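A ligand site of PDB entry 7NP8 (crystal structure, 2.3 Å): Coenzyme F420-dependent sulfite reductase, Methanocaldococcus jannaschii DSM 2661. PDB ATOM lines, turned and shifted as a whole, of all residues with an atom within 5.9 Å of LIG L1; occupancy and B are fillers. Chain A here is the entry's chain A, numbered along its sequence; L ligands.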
ATOM      1  N   ALA A  16      16.271  -3.536 -17.539  1.00  0.00           N
ATOM      2  CA  ALA A  16      16.204  -4.661 -16.598  1.00  0.00           C
ATOM      3  C   ALA A  16      17.207  -4.523 -15.467  1.00  0.00           C
ATOM      4  O   ALA A  16      17.170  -5.337 -14.552  1.00  0.00           O
ATOM      5  CB  ALA A  16      16.464  -5.964 -17.337  1.00  0.00           C
ATOM      6  N   ARG A  17      18.125  -3.539 -15.545  1.00  0.00           N
ATOM      7  CA  ARG A  17      19.158  -3.346 -14.521  1.00  0.00           C
ATOM      8  C   ARG A  17      20.030  -4.603 -14.423  1.00  0.00           C
ATOM      9  O   ARG A  17      20.395  -5.037 -13.327  1.00  0.00           O
ATOM     10  CB  ARG A  17      18.525  -2.993 -13.159  1.00  0.00           C
ATOM     11  CG  ARG A  17      18.086  -1.543 -13.052  1.00  0.00           C
ATOM     12  CD  ARG A  17      17.001  -1.385 -12.005  1.00  0.00           C
ATOM     13  NE  ARG A  17      17.091  -0.108 -11.282  1.00  0.00           N
ATOM     14  CZ  ARG A  17      16.165   0.849 -11.321  1.00  0.00           C
ATOM     15  NH1 ARG A  17      15.062   0.697 -12.050  1.00  0.00           N
ATOM     16  NH2 ARG A  17      16.331   1.966 -10.632  1.00  0.00           N
ATOM     17  N   ARG A  56      16.925  -5.556 -23.647  1.00  0.00           N
ATOM     18  CA  ARG A  56      15.692  -4.790 -23.688  1.00  0.00           C
ATOM     19  C   ARG A  56      15.573  -3.915 -24.939  1.00  0.00           C
ATOM     20  O   ARG A  56      14.538  -3.273 -25.130  1.00  0.00           O
ATOM     21  CB  ARG A  56      15.514  -3.988 -22.392  1.00  0.00           C
ATOM     22  CG  ARG A  56      15.273  -4.874 -21.172  1.00  0.00           C
ATOM     23  CD  ARG A  56      14.034  -5.765 -21.340  1.00  0.00           C
ATOM     24  NE  ARG A  56      14.001  -6.861 -20.377  1.00  0.00           N
ATOM     25  CZ  ARG A  56      13.498  -6.790 -19.156  1.00  0.00           C
ATOM     26  NH1 ARG A  56      13.002  -5.651 -18.692  1.00  0.00           N
ATOM     27  NH2 ARG A  56      13.513  -7.856 -18.358  1.00  0.00           N
ATOM     28  N   LEU A 158      20.575 -13.606 -13.281  1.00  0.00           N
ATOM     29  CA  LEU A 158      19.113 -13.558 -13.343  1.00  0.00           C
ATOM     30  C   LEU A 158      18.745 -13.701 -14.820  1.00  0.00           C
ATOM     31  O   LEU A 158      19.587 -13.441 -15.681  1.00  0.00           O
ATOM     32  CB  LEU A 158      18.598 -12.223 -12.774  1.00  0.00           C
ATOM     33  CG  LEU A 158      19.060 -11.885 -11.355  1.00  0.00           C
ATOM     34  CD1 LEU A 158      18.563 -10.522 -10.944  1.00  0.00           C
ATOM     35  CD2 LEU A 158      18.573 -12.913 -10.362  1.00  0.00           C
ATOM     36  N   PRO A 159      17.519 -14.125 -15.153  1.00  0.00           N
ATOM     37  CA  PRO A 159      17.166 -14.284 -16.578  1.00  0.00           C
ATOM     38  C   PRO A 159      17.607 -13.124 -17.470  1.00  0.00           C
ATOM     39  O   PRO A 159      18.104 -13.373 -18.569  1.00  0.00           O
ATOM     40  CB  PRO A 159      15.644 -14.460 -16.540  1.00  0.00           C
ATOM     41  CG  PRO A 159      15.349 -15.009 -15.190  1.00  0.00           C
ATOM     42  CD  PRO A 159      16.405 -14.491 -14.255  1.00  0.00           C
ATOM     43  N   CYS A 160      17.451 -11.872 -17.016  1.00  0.00           N
ATOM     44  CA  CYS A 160      17.836 -10.693 -17.801  1.00  0.00           C
ATOM     45  C   CYS A 160      19.350 -10.667 -18.068  1.00  0.00           C
ATOM     46  O   CYS A 160      19.780 -10.290 -19.157  1.00  0.00           O
ATOM     47  CB  CYS A 160      17.377  -9.411 -17.111  1.00  0.00           C
ATOM     48  SG  CYS A 160      17.822  -9.319 -15.357  1.00  0.00           S
ATOM     49  N   GLN A 161      20.145 -11.081 -17.067  1.00  0.00           N
ATOM     50  CA  GLN A 161      21.602 -11.121 -17.216  1.00  0.00           C
ATOM     51  C   GLN A 161      22.013 -12.243 -18.157  1.00  0.00           C
ATOM     52  O   GLN A 161      22.913 -12.064 -18.976  1.00  0.00           O
ATOM     53  CB  GLN A 161      22.252 -11.307 -15.831  1.00  0.00           C
ATOM     54  CG  GLN A 161      22.049 -10.097 -14.938  1.00  0.00           C
ATOM     55  CD  GLN A 161      22.529 -10.322 -13.541  1.00  0.00           C
ATOM     56  OE1 GLN A 161      22.372 -11.413 -12.970  1.00  0.00           O
ATOM     57  NE2 GLN A 161      23.107  -9.294 -12.930  1.00  0.00           N
ATOM     58  N   CYS A 201      13.399 -16.210 -11.461  1.00  0.00           N
ATOM     59  CA  CYS A 201      13.332 -14.843 -10.949  1.00  0.00           C
ATOM     60  C   CYS A 201      11.969 -14.237 -11.141  1.00  0.00           C
ATOM     61  O   CYS A 201      11.408 -14.316 -12.227  1.00  0.00           O
ATOM     62  CB  CYS A 201      14.403 -13.990 -11.628  1.00  0.00           C
ATOM     63  SG  CYS A 201      14.569 -12.325 -10.936  1.00  0.00           S
ATOM     64  N   THR A 202      11.437 -13.586 -10.091  1.00  0.00           N
ATOM     65  CA  THR A 202      10.156 -12.887 -10.177  1.00  0.00           C
ATOM     66  C   THR A 202      10.376 -11.388 -10.114  1.00  0.00           C
ATOM     67  O   THR A 202       9.631 -10.645 -10.749  1.00  0.00           O
ATOM     68  CB  THR A 202       9.198 -13.343  -9.068  1.00  0.00           C
ATOM     69  OG1 THR A 202       9.892 -13.386  -7.828  1.00  0.00           O
ATOM     70  CG2 THR A 202       8.559 -14.689  -9.377  1.00  0.00           C
ATOM     71  N   GLU A 203      11.381 -10.934  -9.354  1.00  0.00           N
ATOM     72  CA  GLU A 203      11.657  -9.498  -9.212  1.00  0.00           C
ATOM     73  C   GLU A 203      12.921  -9.247  -8.398  1.00  0.00           C
ATOM     74  O   GLU A 203      13.443 -10.156  -7.751  1.00  0.00           O
ATOM     75  CB  GLU A 203      10.485  -8.789  -8.527  1.00  0.00           C
ATOM     76  CG  GLU A 203      10.005  -9.470  -7.250  1.00  0.00           C
ATOM     77  CD  GLU A 203       8.555  -9.190  -6.920  1.00  0.00           C
ATOM     78  OE1 GLU A 203       7.678  -9.981  -7.339  1.00  0.00           O
ATOM     79  OE2 GLU A 203       8.286  -8.184  -6.225  1.00  0.00           O
ATOM     80  N   LYS A 204      13.397  -7.997  -8.418  1.00  0.00           N
ATOM     81  CA  LYS A 204      14.527  -7.542  -7.617  1.00  0.00           C
ATOM     82  C   LYS A 204      14.197  -6.125  -7.144  1.00  0.00           C
ATOM     83  O   LYS A 204      13.288  -5.497  -7.691  1.00  0.00           O
ATOM     84  CB  LYS A 204      15.848  -7.588  -8.405  1.00  0.00           C
ATOM     85  CG  LYS A 204      15.994  -6.547  -9.503  1.00  0.00           C
ATOM     86  CD  LYS A 204      17.312  -6.715 -10.260  1.00  0.00           C
ATOM     87  CE  LYS A 204      17.263  -6.172 -11.658  1.00  0.00           C
ATOM     88  NZ  LYS A 204      18.107  -6.971 -12.592  1.00  0.00           N
ATOM     89  N   CYS A 253      11.435  -3.050  -9.184  1.00  0.00           N
ATOM     90  CA  CYS A 253      12.123  -2.324 -10.254  1.00  0.00           C
ATOM     91  C   CYS A 253      11.237  -2.305 -11.484  1.00  0.00           C
ATOM     92  O   CYS A 253      10.681  -3.335 -11.855  1.00  0.00           O
ATOM     93  CB  CYS A 253      13.484  -2.947 -10.551  1.00  0.00           C
ATOM     94  SG  CYS A 253      14.711  -2.710  -9.246  1.00  0.00           S
ATOM     95  N   GLY A 255      11.785  -2.335 -14.604  1.00  0.00           N
ATOM     96  CA  GLY A 255      12.174  -3.306 -15.623  1.00  0.00           C
ATOM     97  C   GLY A 255      11.649  -4.707 -15.359  1.00  0.00           C
ATOM     98  O   GLY A 255      11.461  -5.477 -16.301  1.00  0.00           O
ATOM     99  N   CYS A 256      11.422  -5.062 -14.083  1.00  0.00           N
ATOM    100  CA  CYS A 256      10.897  -6.376 -13.715  1.00  0.00           C
ATOM    101  C   CYS A 256       9.461  -6.531 -14.172  1.00  0.00           C
ATOM    102  O   CYS A 256       9.031  -7.640 -14.482  1.00  0.00           O
ATOM    103  CB  CYS A 256      11.030  -6.602 -12.217  1.00  0.00           C
ATOM    104  SG  CYS A 256      12.747  -6.716 -11.641  1.00  0.00           S
ATOM    105  N   LYS A 257       8.711  -5.434 -14.209  1.00  0.00           N
ATOM    106  CA  LYS A 257       7.324  -5.473 -14.682  1.00  0.00           C
ATOM    107  C   LYS A 257       7.287  -5.639 -16.208  1.00  0.00           C
ATOM    108  O   LYS A 257       6.281  -6.091 -16.737  1.00  0.00           O
ATOM    109  CB  LYS A 257       6.578  -4.202 -14.259  1.00  0.00           C
ATOM    110  CG  LYS A 257       5.922  -4.318 -12.891  1.00  0.00           C
ATOM    111  CD  LYS A 257       5.093  -3.099 -12.560  1.00  0.00           C
ATOM    112  CE  LYS A 257       5.936  -1.929 -12.119  1.00  0.00           C
ATOM    113  NZ  LYS A 257       5.647  -0.711 -12.928  1.00  0.00           N
ATOM    114  N   CYS A 259       9.326  -7.719 -17.752  1.00  0.00           N
ATOM    115  CA  CYS A 259      10.042  -8.977 -17.932  1.00  0.00           C
ATOM    116  C   CYS A 259       9.096 -10.127 -18.245  1.00  0.00           C
ATOM    117  O   CYS A 259       8.049 -10.248 -17.611  1.00  0.00           O
ATOM    118  CB  CYS A 259      10.863  -9.284 -16.682  1.00  0.00           C
ATOM    119  SG  CYS A 259      12.071 -10.605 -16.901  1.00  0.00           S
ATOM    120  N   ARG A 260       9.502 -11.016 -19.172  1.00  0.00           N
ATOM    121  CA  ARG A 260       8.728 -12.194 -19.589  1.00  0.00           C
ATOM    122  C   ARG A 260       9.396 -13.510 -19.182  1.00  0.00           C
ATOM    123  O   ARG A 260       8.746 -14.546 -19.205  1.00  0.00           O
ATOM    124  CB  ARG A 260       8.583 -12.193 -21.124  1.00  0.00           C
ATOM    125  CG  ARG A 260       7.782 -11.028 -21.686  1.00  0.00           C
ATOM    126  CD  ARG A 260       8.314 -10.604 -23.044  1.00  0.00           C
ATOM    127  NE  ARG A 260       8.353 -11.702 -24.009  1.00  0.00           N
ATOM    128  CZ  ARG A 260       7.320 -12.090 -24.741  1.00  0.00           C
ATOM    129  NH1 ARG A 260       7.450 -13.100 -25.611  1.00  0.00           N
ATOM    130  NH2 ARG A 260       6.141 -11.498 -24.629  1.00  0.00           N
ATOM    131  N   ASP A 261      10.701 -13.488 -18.867  1.00  0.00           N
ATOM    132  CA  ASP A 261      11.489 -14.692 -18.559  1.00  0.00           C
ATOM    133  C   ASP A 261      11.512 -14.990 -17.068  1.00  0.00           C
ATOM    134  O   ASP A 261      12.174 -14.281 -16.313  1.00  0.00           O
ATOM    135  CB  ASP A 261      12.920 -14.486 -19.092  1.00  0.00           C
ATOM    136  CG  ASP A 261      13.713 -15.761 -19.338  1.00  0.00           C
ATOM    137  OD1 ASP A 261      13.361 -16.799 -18.741  1.00  0.00           O
ATOM    138  OD2 ASP A 261      14.699 -15.709 -20.106  1.00  0.00           O
ATOM    139  N   LYS A 315       4.038 -14.243 -14.352  1.00  0.00           N
ATOM    140  CA  LYS A 315       5.012 -13.265 -14.809  1.00  0.00           C
ATOM    141  C   LYS A 315       4.598 -12.675 -16.165  1.00  0.00           C
ATOM    142  O   LYS A 315       4.794 -11.490 -16.402  1.00  0.00           O
ATOM    143  CB  LYS A 315       6.406 -13.894 -14.902  1.00  0.00           C
ATOM    144  CG  LYS A 315       7.510 -12.873 -15.169  1.00  0.00           C
ATOM    145  CD  LYS A 315       8.864 -13.371 -14.709  1.00  0.00           C
ATOM    146  CE  LYS A 315       9.886 -12.279 -14.752  1.00  0.00           C
ATOM    147  NZ  LYS A 315      11.213 -12.744 -14.305  1.00  0.00           N
ATOM    148  N   ARG A 318       1.677 -10.242 -15.616  1.00  0.00           N
ATOM    149  CA  ARG A 318       2.201  -8.994 -15.066  1.00  0.00           C
ATOM    150  C   ARG A 318       2.848  -8.186 -16.183  1.00  0.00           C
ATOM    151  O   ARG A 318       2.726  -6.958 -16.199  1.00  0.00           O
ATOM    152  CB  ARG A 318       3.213  -9.295 -13.954  1.00  0.00           C
ATOM    153  CG  ARG A 318       3.739  -8.050 -13.275  1.00  0.00           C
ATOM    154  CD  ARG A 318       4.761  -8.400 -12.220  1.00  0.00           C
ATOM    155  NE  ARG A 318       6.033  -8.800 -12.828  1.00  0.00           N
ATOM    156  CZ  ARG A 318       7.069  -9.277 -12.147  1.00  0.00           C
ATOM    157  NH1 ARG A 318       6.992  -9.409 -10.828  1.00  0.00           N
ATOM    158  NH2 ARG A 318       8.185  -9.617 -12.777  1.00  0.00           N
HETATM  159 FE1  LIG L   1      13.225  -9.952 -15.006  1.00  0.00          FE
HETATM  160 FE2  LIG L   1      13.652  -8.307 -12.934  1.00  0.00          FE
HETATM  161 FE3  LIG L   1      15.728  -9.342 -14.337  1.00  0.00          FE
HETATM  162 FE4  LIG L   1      14.199 -10.895 -12.654  1.00  0.00          FE
HETATM  163  S1  LIG L   1      15.587  -9.136 -12.016  1.00  0.00           S
HETATM  164  S2  LIG L   1      14.951 -11.476 -14.777  1.00  0.00           S
HETATM  165  S3  LIG L   1      12.077 -10.018 -12.965  1.00  0.00           S
HETATM  166  S4  LIG L   1      14.182  -7.857 -15.152  1.00  0.00           S
HETATM  167  P1  LG2 L   2      23.153 -21.245  -3.829  1.00  0.00           P
HETATM  168  O1  LG2 L   2      23.973 -22.484  -3.764  1.00  0.00           O
HETATM  169  O2  LG2 L   2      22.730 -20.589  -2.562  1.00  0.00           O
HETATM  170  O3  LG2 L   2      23.892 -20.178  -4.759  1.00  0.00           O
HETATM  171  C1  LG2 L   2      23.261 -18.907  -4.999  1.00  0.00           C
HETATM  172  C2  LG2 L   2      23.876 -18.268  -6.214  1.00  0.00           C
HETATM  173  O4  LG2 L   2      23.057 -17.157  -6.627  1.00  0.00           O
HETATM  174  C3  LG2 L   2      25.300 -17.708  -6.033  1.00  0.00           C
HETATM  175  O5  LG2 L   2      26.214 -18.322  -6.921  1.00  0.00           O
HETATM  176  C4  LG2 L   2      25.162 -16.204  -6.265  1.00  0.00           C
HETATM  177  O6  LG2 L   2      26.256 -15.690  -6.996  1.00  0.00           O
HETATM  178  C5  LG2 L   2      23.856 -16.086  -7.051  1.00  0.00           C
HETATM  179  N1  LG2 L   2      23.123 -14.860  -6.791  1.00  0.00           N
HETATM  180  C6  LG2 L   2      22.554 -14.481  -5.608  1.00  0.00           C
HETATM  181  N2  LG2 L   2      21.953 -13.319  -5.691  1.00  0.00           N
HETATM  182  C7  LG2 L   2      22.124 -12.928  -7.009  1.00  0.00           C
HETATM  183  C8  LG2 L   2      21.711 -11.790  -7.723  1.00  0.00           C
HETATM  184  N3  LG2 L   2      21.015 -10.797  -7.194  1.00  0.00           N
HETATM  185  N4  LG2 L   2      22.056 -11.722  -9.031  1.00  0.00           N
HETATM  186  C9  LG2 L   2      22.763 -12.722  -9.558  1.00  0.00           C
HETATM  187  N5  LG2 L   2      23.198 -13.837  -8.989  1.00  0.00           N
HETATM  188  C10 LG2 L   2      22.848 -13.879  -7.694  1.00  0.00           C
HETATM  189  N6  LG2 L   2      13.477 -18.882  -7.365  1.00  0.00           N
HETATM  190  C11 LG2 L   2      12.175 -19.185  -7.516  1.00  0.00           C
HETATM  191  O7  LG2 L   2      11.803 -20.356  -7.585  1.00  0.00           O
HETATM  192  N7  LG2 L   2      11.214 -18.241  -7.610  1.00  0.00           N
HETATM  193  C12 LG2 L   2      11.518 -16.910  -7.555  1.00  0.00           C
HETATM  194  O8  LG2 L   2      10.620 -16.086  -7.644  1.00  0.00           O
HETATM  195  C13 LG2 L   2      12.859 -16.536  -7.393  1.00  0.00           C
HETATM  196  N8  LG2 L   2      13.168 -15.272  -7.338  1.00  0.00           N
HETATM  197  C14 LG2 L   2      14.477 -14.946  -7.190  1.00  0.00           C
HETATM  198  C15 LG2 L   2      14.831 -13.580  -7.131  1.00  0.00           C
HETATM  199  C16 LG2 L   2      16.135 -13.186  -6.984  1.00  0.00           C
HETATM  200  C17 LG2 L   2      16.469 -11.715  -6.932  1.00  0.00           C
HETATM  201  C18 LG2 L   2      17.153 -14.158  -6.876  1.00  0.00           C
HETATM  202  C19 LG2 L   2      18.587 -13.736  -6.704  1.00  0.00           C
HETATM  203  C20 LG2 L   2      16.830 -15.490  -6.926  1.00  0.00           C
HETATM  204  C21 LG2 L   2      15.495 -15.917  -7.083  1.00  0.00           C
HETATM  205  N9  LG2 L   2      15.128 -17.253  -7.144  1.00  0.00           N
HETATM  206  C22 LG2 L   2      13.809 -17.621  -7.302  1.00  0.00           C
HETATM  207  C23 LG2 L   2      16.169 -18.295  -7.050  1.00  0.00           C
HETATM  208  C24 LG2 L   2      16.343 -18.832  -5.647  1.00  0.00           C
HETATM  209  O9  LG2 L   2      16.259 -17.778  -4.706  1.00  0.00           O
HETATM  210  C25 LG2 L   2      17.699 -19.512  -5.507  1.00  0.00           C
HETATM  211  O10 LG2 L   2      18.714 -18.556  -5.776  1.00  0.00           O
HETATM  212  C26 LG2 L   2      17.897 -20.700  -6.446  1.00  0.00           C
HETATM  213  O11 LG2 L   2      16.876 -21.669  -6.203  1.00  0.00           O
HETATM  214  C27 LG2 L   2      19.250 -21.352  -6.273  1.00  0.00           C
HETATM  215  O12 LG2 L   2      19.388 -21.785  -4.896  1.00  0.00           O
HETATM  216  P2  LG2 L   2      20.678 -22.616  -4.461  1.00  0.00           P
HETATM  217  O13 LG2 L   2      20.578 -22.910  -3.003  1.00  0.00           O
HETATM  218  O14 LG2 L   2      20.881 -23.750  -5.408  1.00  0.00           O
HETATM  219  O15 LG2 L   2      21.842 -21.550  -4.684  1.00  0.00           O
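The backbone carbonyl oxygen (O) of Thr 202 lies within hydrogen-bond range of the guanidinium group (NH2) of Arg 318 (2.7 Å). The backbone carbonyl oxygen (O) of Gly 255 lies within hydrogen-bond range of the guanidinium group (NH1) of Arg 56 (2.8 Å). The backbone carbonyl oxygen of Lys 204 sits at hydrogen-bond distance from the backbone NH of Cys 253, at 3.4 Å. N of Leu 158 lies within hydrogen-bond range of OE1 of Gln 161 (2.9 Å). The backbone carbonyl oxygen (O) of Cys 256 sits at hydrogen-bond distance from the guanidinium group (NH2) of Arg 318 (2.7 Å). N of Lys 204 sits close to SG of Cys 256, at 3.5 Å. The side-chain sulfur (SG) of Cys 259 sits close to the guanidinium group (NH2) of Arg 56. The backbone carbonyl oxygen (O) of Ala 16 is in hydrogen-bond range of the side-chain amino group (NZ) of Lys 204 (2.7 Å).
NH2 of Arg 56 sits close to S4 of LIG L1 (3.3 Å). An oxygen (O8) of LG2 L2 sits at hydrogen-bond distance from the side-chain hydroxyl of Thr 202. A sulfur (S1) of LIG L1 lies close to the side-chain amino group (NZ) of Lys 204 (3.4 Å). SG of Cys 160 binds FE3 of LIG L1, at 2.3 Å. The side-chain sulfur of Cys 256 binds an iron atom (FE2) of LIG L1. A sulfur (S3) of LIG L1 lies close to the backbone NH (N) of Glu 203 (3.8 Å). The side-chain sulfur of Cys 259 binds an iron atom (FE1) of LIG L1, at 2.3 Å. FE4 of LIG L1 is bound by SG of Cys 201 (2.3 Å). The backbone NH (N) of Cys 160 sits close to a sulfur (S2) of LIG L1, 3.4 Å away. The side-chain amino group (NZ) of Lys 315 lies close to a sulfur (S3) of LIG L1, 3.2 Å away.
The backbone nitrogen (N) of Pro 159 lies close to a sulfur (S2) of LIG L1. S3 of LIG L1 sits close to O of Thr 202. O of Gly 255 lies close to S4 of LIG L1, at 3.8 Å. Ala 16 touches LIG L1. CD1 of Leu 158 touches S1 of LIG L1, at 3.5 Å. Arg 318 touches LIG L1 (NH2 to S3, 3.9 Å). The nearest printed residue that does not touch LIG L1 is Asp 261 (4.2 Å).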
